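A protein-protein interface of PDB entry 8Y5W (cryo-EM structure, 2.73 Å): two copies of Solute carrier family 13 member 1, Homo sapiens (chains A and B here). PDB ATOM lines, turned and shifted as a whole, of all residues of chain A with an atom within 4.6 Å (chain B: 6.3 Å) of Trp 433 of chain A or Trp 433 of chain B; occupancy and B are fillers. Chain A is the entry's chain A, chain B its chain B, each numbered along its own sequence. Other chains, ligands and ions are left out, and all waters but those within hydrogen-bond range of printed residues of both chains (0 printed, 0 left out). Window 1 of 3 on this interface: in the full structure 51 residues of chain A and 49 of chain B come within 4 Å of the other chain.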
ATOM      1  N   PHE A 427     -14.748  -6.291  10.836  1.00  0.00           N
ATOM      2  CA  PHE A 427     -13.421  -6.084  11.406  1.00  0.00           C
ATOM      3  C   PHE A 427     -12.343  -5.987  10.337  1.00  0.00           C
ATOM      4  O   PHE A 427     -11.372  -5.244  10.512  1.00  0.00           O
ATOM      5  CB  PHE A 427     -13.074  -7.215  12.376  1.00  0.00           C
ATOM      6  CG  PHE A 427     -11.631  -7.230  12.789  1.00  0.00           C
ATOM      7  CD1 PHE A 427     -11.165  -6.360  13.756  1.00  0.00           C
ATOM      8  CD2 PHE A 427     -10.734  -8.101  12.193  1.00  0.00           C
ATOM      9  CE1 PHE A 427      -9.837  -6.366  14.130  1.00  0.00           C
ATOM     10  CE2 PHE A 427      -9.405  -8.107  12.563  1.00  0.00           C
ATOM     11  CZ  PHE A 427      -8.957  -7.241  13.532  1.00  0.00           C
ATOM     12  N   GLN A 428     -12.479  -6.743   9.245  1.00  0.00           N
ATOM     13  CA  GLN A 428     -11.475  -6.704   8.187  1.00  0.00           C
ATOM     14  C   GLN A 428     -11.398  -5.319   7.562  1.00  0.00           C
ATOM     15  O   GLN A 428     -10.308  -4.842   7.225  1.00  0.00           O
ATOM     16  CB  GLN A 428     -11.781  -7.769   7.136  1.00  0.00           C
ATOM     17  CG  GLN A 428     -10.625  -8.071   6.201  1.00  0.00           C
ATOM     18  CD  GLN A 428     -10.855  -9.320   5.379  1.00  0.00           C
ATOM     19  OE1 GLN A 428     -11.893  -9.970   5.493  1.00  0.00           O
ATOM     20  NE2 GLN A 428      -9.886  -9.662   4.542  1.00  0.00           N
ATOM     21  N   MET A 431      -9.492  -2.217   9.726  1.00  0.00           N
ATOM     22  CA  MET A 431      -8.272  -2.771  10.299  1.00  0.00           C
ATOM     23  C   MET A 431      -7.070  -2.301   9.491  1.00  0.00           C
ATOM     24  O   MET A 431      -6.991  -2.592   8.293  1.00  0.00           O
ATOM     25  CB  MET A 431      -8.334  -4.291  10.315  1.00  0.00           C
ATOM     26  CG  MET A 431      -7.023  -4.971  10.665  1.00  0.00           C
ATOM     27  SD  MET A 431      -6.432  -4.615  12.328  1.00  0.00           S
ATOM     28  CE  MET A 431      -4.695  -4.994  12.144  1.00  0.00           C
ATOM     29  N   PRO A 432      -6.127  -1.579  10.092  1.00  0.00           N
ATOM     30  CA  PRO A 432      -4.985  -1.072   9.322  1.00  0.00           C
ATOM     31  C   PRO A 432      -3.990  -2.162   8.958  1.00  0.00           C
ATOM     32  O   PRO A 432      -2.952  -2.300   9.610  1.00  0.00           O
ATOM     33  CB  PRO A 432      -4.356  -0.038  10.265  1.00  0.00           C
ATOM     34  CG  PRO A 432      -5.385   0.215  11.328  1.00  0.00           C
ATOM     35  CD  PRO A 432      -6.121  -1.070  11.471  1.00  0.00           C
ATOM     36  N   TRP A 433      -4.301  -2.946   7.924  1.00  0.00           N
ATOM     37  CA  TRP A 433      -3.349  -3.935   7.432  1.00  0.00           C
ATOM     38  C   TRP A 433      -2.098  -3.283   6.864  1.00  0.00           C
ATOM     39  O   TRP A 433      -0.993  -3.812   7.047  1.00  0.00           O
ATOM     40  CB  TRP A 433      -4.005  -4.813   6.368  1.00  0.00           C
ATOM     41  CG  TRP A 433      -5.254  -5.493   6.829  1.00  0.00           C
ATOM     42  CD1 TRP A 433      -6.530  -5.203   6.450  1.00  0.00           C
ATOM     43  CD2 TRP A 433      -5.348  -6.581   7.754  1.00  0.00           C
ATOM     44  NE1 TRP A 433      -7.414  -6.040   7.081  1.00  0.00           N
ATOM     45  CE2 TRP A 433      -6.713  -6.897   7.887  1.00  0.00           C
ATOM     46  CE3 TRP A 433      -4.410  -7.319   8.481  1.00  0.00           C
ATOM     47  CZ2 TRP A 433      -7.163  -7.916   8.719  1.00  0.00           C
ATOM     48  CZ3 TRP A 433      -4.859  -8.331   9.305  1.00  0.00           C
ATOM     49  CH2 TRP A 433      -6.223  -8.620   9.418  1.00  0.00           C
ATOM     50  N   ASP A 434      -2.252  -2.146   6.182  1.00  0.00           N
ATOM     51  CA  ASP A 434      -1.096  -1.426   5.661  1.00  0.00           C
ATOM     52  C   ASP A 434      -0.179  -0.967   6.785  1.00  0.00           C
ATOM     53  O   ASP A 434       1.047  -1.069   6.672  1.00  0.00           O
ATOM     54  CB  ASP A 434      -1.555  -0.236   4.819  1.00  0.00           C
ATOM     55  CG  ASP A 434      -2.530   0.661   5.556  1.00  0.00           C
ATOM     56  OD1 ASP A 434      -3.429   0.133   6.241  1.00  0.00           O
ATOM     57  OD2 ASP A 434      -2.397   1.898   5.449  1.00  0.00           O
ATOM     58  N   ILE A 435      -0.751  -0.466   7.882  1.00  0.00           N
ATOM     59  CA  ILE A 435       0.064  -0.050   9.018  1.00  0.00           C
ATOM     60  C   ILE A 435       0.739  -1.249   9.667  1.00  0.00           C
ATOM     61  O   ILE A 435       1.895  -1.161  10.100  1.00  0.00           O
ATOM     62  CB  ILE A 435      -0.792   0.736  10.028  1.00  0.00           C
ATOM     63  CG1 ILE A 435      -1.370   1.984   9.364  1.00  0.00           C
ATOM     64  CG2 ILE A 435       0.025   1.117  11.250  1.00  0.00           C
ATOM     65  CD1 ILE A 435      -0.314   2.933   8.846  1.00  0.00           C
ATOM     66  N   ALA A 436       0.044  -2.386   9.747  1.00  0.00           N
ATOM     67  CA  ALA A 436       0.659  -3.590  10.289  1.00  0.00           C
ATOM     68  C   ALA A 436       1.867  -4.020   9.469  1.00  0.00           C
ATOM     69  O   ALA A 436       2.931  -4.306  10.034  1.00  0.00           O
ATOM     70  CB  ALA A 436      -0.367  -4.720  10.353  1.00  0.00           C
ATOM     71  N   ILE A 437       1.735  -4.044   8.145  1.00  0.00           N
ATOM     72  CA  ILE A 437       2.856  -4.407   7.283  1.00  0.00           C
ATOM     73  C   ILE A 437       3.973  -3.371   7.354  1.00  0.00           C
ATOM     74  O   ILE A 437       5.152  -3.725   7.336  1.00  0.00           O
ATOM     75  CB  ILE A 437       2.364  -4.618   5.838  1.00  0.00           C
ATOM     76  CG1 ILE A 437       1.475  -5.858   5.766  1.00  0.00           C
ATOM     77  CG2 ILE A 437       3.535  -4.757   4.881  1.00  0.00           C
ATOM     78  CD1 ILE A 437       0.881  -6.095   4.408  1.00  0.00           C
ATOM     79  N   SER B  56     -10.905 -17.138  11.622  1.00  0.00           N
ATOM     80  CA  SER B  56      -9.826 -16.228  11.976  1.00  0.00           C
ATOM     81  C   SER B  56      -9.895 -15.778  13.429  1.00  0.00           C
ATOM     82  O   SER B  56      -8.851 -15.490  14.022  1.00  0.00           O
ATOM     83  CB  SER B  56      -9.846 -15.012  11.053  1.00  0.00           C
ATOM     84  OG  SER B  56      -9.686 -15.401   9.702  1.00  0.00           O
ATOM     85  N   ILE B  90       1.643 -13.009  -0.035  1.00  0.00           N
ATOM     86  CA  ILE B  90       1.629 -11.622  -0.490  1.00  0.00           C
ATOM     87  C   ILE B  90       2.051 -11.540  -1.950  1.00  0.00           C
ATOM     88  O   ILE B  90       1.405 -10.865  -2.760  1.00  0.00           O
ATOM     89  CB  ILE B  90       2.522 -10.751   0.413  1.00  0.00           C
ATOM     90  CG1 ILE B  90       1.865 -10.552   1.778  1.00  0.00           C
ATOM     91  CG2 ILE B  90       2.791  -9.405  -0.237  1.00  0.00           C
ATOM     92  CD1 ILE B  90       2.803 -10.011   2.832  1.00  0.00           C
ATOM     93  N   TRP B 424      -2.096  -0.246  -3.932  1.00  0.00           N
ATOM     94  CA  TRP B 424      -2.215  -0.865  -2.617  1.00  0.00           C
ATOM     95  C   TRP B 424      -3.669  -0.954  -2.177  1.00  0.00           C
ATOM     96  O   TRP B 424      -4.040  -1.871  -1.439  1.00  0.00           O
ATOM     97  CB  TRP B 424      -1.401  -0.108  -1.572  1.00  0.00           C
ATOM     98  CG  TRP B 424      -1.497  -0.781  -0.244  1.00  0.00           C
ATOM     99  CD1 TRP B 424      -2.344  -0.465   0.776  1.00  0.00           C
ATOM    100  CD2 TRP B 424      -0.754  -1.925   0.190  1.00  0.00           C
ATOM    101  NE1 TRP B 424      -2.161  -1.329   1.826  1.00  0.00           N
ATOM    102  CE2 TRP B 424      -1.190  -2.235   1.492  1.00  0.00           C
ATOM    103  CE3 TRP B 424       0.246  -2.709  -0.391  1.00  0.00           C
ATOM    104  CZ2 TRP B 424      -0.661  -3.294   2.222  1.00  0.00           C
ATOM    105  CZ3 TRP B 424       0.770  -3.759   0.334  1.00  0.00           C
ATOM    106  CH2 TRP B 424       0.315  -4.042   1.626  1.00  0.00           C
ATOM    107  N   PHE B 427      -4.905  -4.015  -3.655  1.00  0.00           N
ATOM    108  CA  PHE B 427      -4.278  -5.197  -3.076  1.00  0.00           C
ATOM    109  C   PHE B 427      -4.798  -5.508  -1.677  1.00  0.00           C
ATOM    110  O   PHE B 427      -4.927  -6.682  -1.317  1.00  0.00           O
ATOM    111  CB  PHE B 427      -2.758  -5.025  -3.025  1.00  0.00           C
ATOM    112  CG  PHE B 427      -2.058  -6.084  -2.222  1.00  0.00           C
ATOM    113  CD1 PHE B 427      -1.830  -7.340  -2.755  1.00  0.00           C
ATOM    114  CD2 PHE B 427      -1.640  -5.828  -0.927  1.00  0.00           C
ATOM    115  CE1 PHE B 427      -1.195  -8.315  -2.016  1.00  0.00           C
ATOM    116  CE2 PHE B 427      -1.005  -6.800  -0.185  1.00  0.00           C
ATOM    117  CZ  PHE B 427      -0.781  -8.044  -0.732  1.00  0.00           C
ATOM    118  N   GLN B 428      -5.087  -4.478  -0.877  1.00  0.00           N
ATOM    119  CA  GLN B 428      -5.588  -4.704   0.475  1.00  0.00           C
ATOM    120  C   GLN B 428      -6.928  -5.425   0.447  1.00  0.00           C
ATOM    121  O   GLN B 428      -7.149  -6.368   1.216  1.00  0.00           O
ATOM    122  CB  GLN B 428      -5.695  -3.375   1.219  1.00  0.00           C
ATOM    123  CG  GLN B 428      -5.829  -3.516   2.723  1.00  0.00           C
ATOM    124  CD  GLN B 428      -5.681  -2.192   3.438  1.00  0.00           C
ATOM    125  OE1 GLN B 428      -5.533  -1.148   2.807  1.00  0.00           O
ATOM    126  NE2 GLN B 428      -5.715  -2.229   4.763  1.00  0.00           N
ATOM    127  N   SER B 429      -7.835  -4.994  -0.422  1.00  0.00           N
ATOM    128  CA  SER B 429      -8.935  -5.849  -0.833  1.00  0.00           C
ATOM    129  C   SER B 429      -8.404  -6.874  -1.824  1.00  0.00           C
ATOM    130  O   SER B 429      -7.402  -6.638  -2.502  1.00  0.00           O
ATOM    131  CB  SER B 429     -10.063  -5.029  -1.457  1.00  0.00           C
ATOM    132  OG  SER B 429      -9.631  -4.389  -2.643  1.00  0.00           O
ATOM    133  N   PHE B 430      -9.070  -8.025  -1.893  1.00  0.00           N
ATOM    134  CA  PHE B 430      -8.668  -9.221  -2.625  1.00  0.00           C
ATOM    135  C   PHE B 430      -7.549  -9.961  -1.886  1.00  0.00           C
ATOM    136  O   PHE B 430      -7.246 -11.099  -2.243  1.00  0.00           O
ATOM    137  CB  PHE B 430      -8.226  -8.924  -4.075  1.00  0.00           C
ATOM    138  CG  PHE B 430      -7.990 -10.144  -4.917  1.00  0.00           C
ATOM    139  CD1 PHE B 430      -9.046 -10.796  -5.526  1.00  0.00           C
ATOM    140  CD2 PHE B 430      -6.708 -10.622  -5.121  1.00  0.00           C
ATOM    141  CE1 PHE B 430      -8.830 -11.911  -6.306  1.00  0.00           C
ATOM    142  CE2 PHE B 430      -6.489 -11.738  -5.895  1.00  0.00           C
ATOM    143  CZ  PHE B 430      -7.549 -12.382  -6.492  1.00  0.00           C
ATOM    144  N   MET B 431      -6.968  -9.383  -0.845  1.00  0.00           N
ATOM    145  CA  MET B 431      -6.000 -10.092  -0.015  1.00  0.00           C
ATOM    146  C   MET B 431      -6.724 -10.950   1.014  1.00  0.00           C
ATOM    147  O   MET B 431      -7.536 -10.429   1.785  1.00  0.00           O
ATOM    148  CB  MET B 431      -5.071  -9.112   0.690  1.00  0.00           C
ATOM    149  CG  MET B 431      -3.937  -9.764   1.466  1.00  0.00           C
ATOM    150  SD  MET B 431      -2.714 -10.647   0.492  1.00  0.00           S
ATOM    151  CE  MET B 431      -2.079 -11.774   1.726  1.00  0.00           C
ATOM    152  N   PRO B 432      -6.466 -12.253   1.054  1.00  0.00           N
ATOM    153  CA  PRO B 432      -7.085 -13.091   2.085  1.00  0.00           C
ATOM    154  C   PRO B 432      -6.491 -12.826   3.457  1.00  0.00           C
ATOM    155  O   PRO B 432      -5.712 -13.638   3.966  1.00  0.00           O
ATOM    156  CB  PRO B 432      -6.783 -14.519   1.610  1.00  0.00           C
ATOM    157  CG  PRO B 432      -6.348 -14.381   0.182  1.00  0.00           C
ATOM    158  CD  PRO B 432      -5.686 -13.052   0.100  1.00  0.00           C
ATOM    159  N   TRP B 433      -6.840 -11.689   4.060  1.00  0.00           N
ATOM    160  CA  TRP B 433      -6.414 -11.425   5.427  1.00  0.00           C
ATOM    161  C   TRP B 433      -7.013 -12.424   6.403  1.00  0.00           C
ATOM    162  O   TRP B 433      -6.492 -12.582   7.512  1.00  0.00           O
ATOM    163  CB  TRP B 433      -6.791 -10.001   5.835  1.00  0.00           C
ATOM    164  CG  TRP B 433      -6.180  -8.944   4.969  1.00  0.00           C
ATOM    165  CD1 TRP B 433      -6.831  -8.120   4.103  1.00  0.00           C
ATOM    166  CD2 TRP B 433      -4.793  -8.600   4.885  1.00  0.00           C
ATOM    167  NE1 TRP B 433      -5.939  -7.280   3.486  1.00  0.00           N
ATOM    168  CE2 TRP B 433      -4.680  -7.554   3.949  1.00  0.00           C
ATOM    169  CE3 TRP B 433      -3.637  -9.070   5.513  1.00  0.00           C
ATOM    170  CZ2 TRP B 433      -3.458  -6.975   3.623  1.00  0.00           C
ATOM    171  CZ3 TRP B 433      -2.426  -8.494   5.188  1.00  0.00           C
ATOM    172  CH2 TRP B 433      -2.346  -7.457   4.252  1.00  0.00           C
ATOM    173  N   ASP B 434      -8.099 -13.093   6.011  1.00  0.00           N
ATOM    174  CA  ASP B 434      -8.629 -14.196   6.802  1.00  0.00           C
ATOM    175  C   ASP B 434      -7.618 -15.326   6.893  1.00  0.00           C
ATOM    176  O   ASP B 434      -7.294 -15.806   7.986  1.00  0.00           O
ATOM    177  CB  ASP B 434      -9.913 -14.718   6.163  1.00  0.00           C
ATOM    178  CG  ASP B 434     -11.025 -13.712   6.198  1.00  0.00           C
ATOM    179  OD1 ASP B 434     -11.023 -12.879   7.116  1.00  0.00           O
ATOM    180  OD2 ASP B 434     -11.898 -13.756   5.306  1.00  0.00           O
ATOM    181  N   ILE B 435      -7.109 -15.759   5.741  1.00  0.00           N
ATOM    182  CA  ILE B 435      -6.227 -16.913   5.664  1.00  0.00           C
ATOM    183  C   ILE B 435      -4.870 -16.625   6.287  1.00  0.00           C
ATOM    184  O   ILE B 435      -4.264 -17.516   6.885  1.00  0.00           O
ATOM    185  CB  ILE B 435      -6.109 -17.362   4.200  1.00  0.00           C
ATOM    186  CG1 ILE B 435      -7.474 -17.837   3.709  1.00  0.00           C
ATOM    187  CG2 ILE B 435      -5.055 -18.440   4.038  1.00  0.00           C
ATOM    188  CD1 ILE B 435      -8.056 -18.967   4.525  1.00  0.00           C
ATOM    189  N   ALA B 436      -4.363 -15.398   6.157  1.00  0.00           N
ATOM    190  CA  ALA B 436      -3.116 -15.058   6.832  1.00  0.00           C
ATOM    191  C   ALA B 436      -3.218 -15.295   8.333  1.00  0.00           C
ATOM    192  O   ALA B 436      -2.366 -15.977   8.913  1.00  0.00           O
ATOM    193  CB  ALA B 436      -2.741 -13.604   6.545  1.00  0.00           C
ATOM    194  N   ILE B 437      -4.275 -14.784   8.963  1.00  0.00           N
ATOM    195  CA  ILE B 437      -4.458 -14.965  10.399  1.00  0.00           C
ATOM    196  C   ILE B 437      -4.750 -16.423  10.733  1.00  0.00           C
ATOM    197  O   ILE B 437      -4.290 -16.935  11.757  1.00  0.00           O
ATOM    198  CB  ILE B 437      -5.564 -14.023  10.910  1.00  0.00           C
ATOM    199  CG1 ILE B 437      -5.061 -12.581  10.917  1.00  0.00           C
ATOM    200  CG2 ILE B 437      -6.027 -14.425  12.302  1.00  0.00           C
ATOM    201  CD1 ILE B 437      -6.111 -11.576  11.293  1.00  0.00           C
ATOM    202  N   LEU B 438      -5.510 -17.117   9.883  1.00  0.00           N
ATOM    203  CA  LEU B 438      -5.820 -18.520  10.147  1.00  0.00           C
ATOM    204  C   LEU B 438      -4.562 -19.385  10.138  1.00  0.00           C
ATOM    205  O   LEU B 438      -4.342 -20.190  11.054  1.00  0.00           O
ATOM    206  CB  LEU B 438      -6.828 -19.023   9.115  1.00  0.00           C
ATOM    207  CG  LEU B 438      -7.350 -20.449   9.271  1.00  0.00           C
ATOM    208  CD1 LEU B 438      -8.265 -20.546  10.474  1.00  0.00           C
ATOM    209  CD2 LEU B 438      -8.070 -20.890   8.009  1.00  0.00           C
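O of Met 431 of chain B touches NE2 of Gln 428 of chain A, 3.7 Å away. Trp 433 of chain B touches Gln 428 of chain A (CB to NE2, 3.4 Å). Gln 428 of chain B touches Met 431 of chain A (NE2 to O, 3.8 Å). CB of Trp 433 of chain A touches NE2 of Gln 428 of chain B (3.5 Å). CE3 of Trp 433 of chain A touches CE3 of Trp 433 of chain B, 3.5 Å away. Trp 433 of chain A touches Ile 437 of chain B (CH2 to CD1, 3.5 Å). Trp 424 of chain B touches Asp 434 of chain A. Asp 434 of chain A touches Gln 428 of chain B. Ile 437 of chain A touches Trp 424 of chain B (CD1 to CH2, 3.5 Å). Ile 437 of chain A touches Trp 433 of chain B (CD1 to CH2, 3.5 Å).
Trp 433 of chain A touches just these residues of chain B: Gln 428 (3.5 Å), Trp 433 (3.5 Å) and Ile 437 (3.5 Å). Trp 433 of chain B touches three residues of chain A. Printed residues of chain A within 4 Å of Ile 437 of chain B: Trp 433. Of the printed residues of chain B, Asp 434 of chain A touches Trp 424 (3.2 Å) and Gln 428 (3.6 Å). The nearest printed residue of chain A that does not touch Gln 428 of chain B is Pro 432 of chain A (4.5 Å).
Gln 428 of chain A touches Met 431 of chain B, and with the chains exchanged Met 431 of chain A touches Gln 428 of chain B. Gln 428 of chain A touches Asp 434 of chain B, and with the chains exchanged Asp 434 of chain A touches Gln 428 of chain B. Trp 433 of chain B touches its own counterpart, Trp 433 of chain A. Trp 433 of chain A touches Ile 437 of chain B, and with the chains exchanged Ile 437 of chain A touches Trp 433 of chain B. 9 positions are printed for both chains. Of the 11 pairs that touch across the chains among the printed residues, 9 have their exchanged pair printed and touching as well.
Hydrophobic or aromatic side chains of chain A within 4 Å of the printed part of chain B: Trp 433 and Ile 437. Of the 15 printed residues of chain B, 6 touch a printed residue of chain A. Among the printed residues, 11 pairs touch across the chains. Among the printed residues, no Asp or Glu carboxylate lies within 4 Å of a Lys or Arg side-chain nitrogen of the other chain.
O of Gln 428 of chain B sits at hydrogen-bond distance from NE1 of Trp 433 of chain B. O of Asp 434 of chain B sits at hydrogen-bond distance from OG of Ser 56 of chain B, at 3.0 Å. The backbone carbonyl oxygen (O) of Gln 428 of chain A is in hydrogen-bond range of the indole nitrogen (NE1) of Trp 433 of chain A (3.1 Å).
The side-chain amide oxygen (OE1) of Gln 428 of chain A sits close to the side-chain carboxylate (OD1) of Asp 434 of chain B (3.4 Å).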
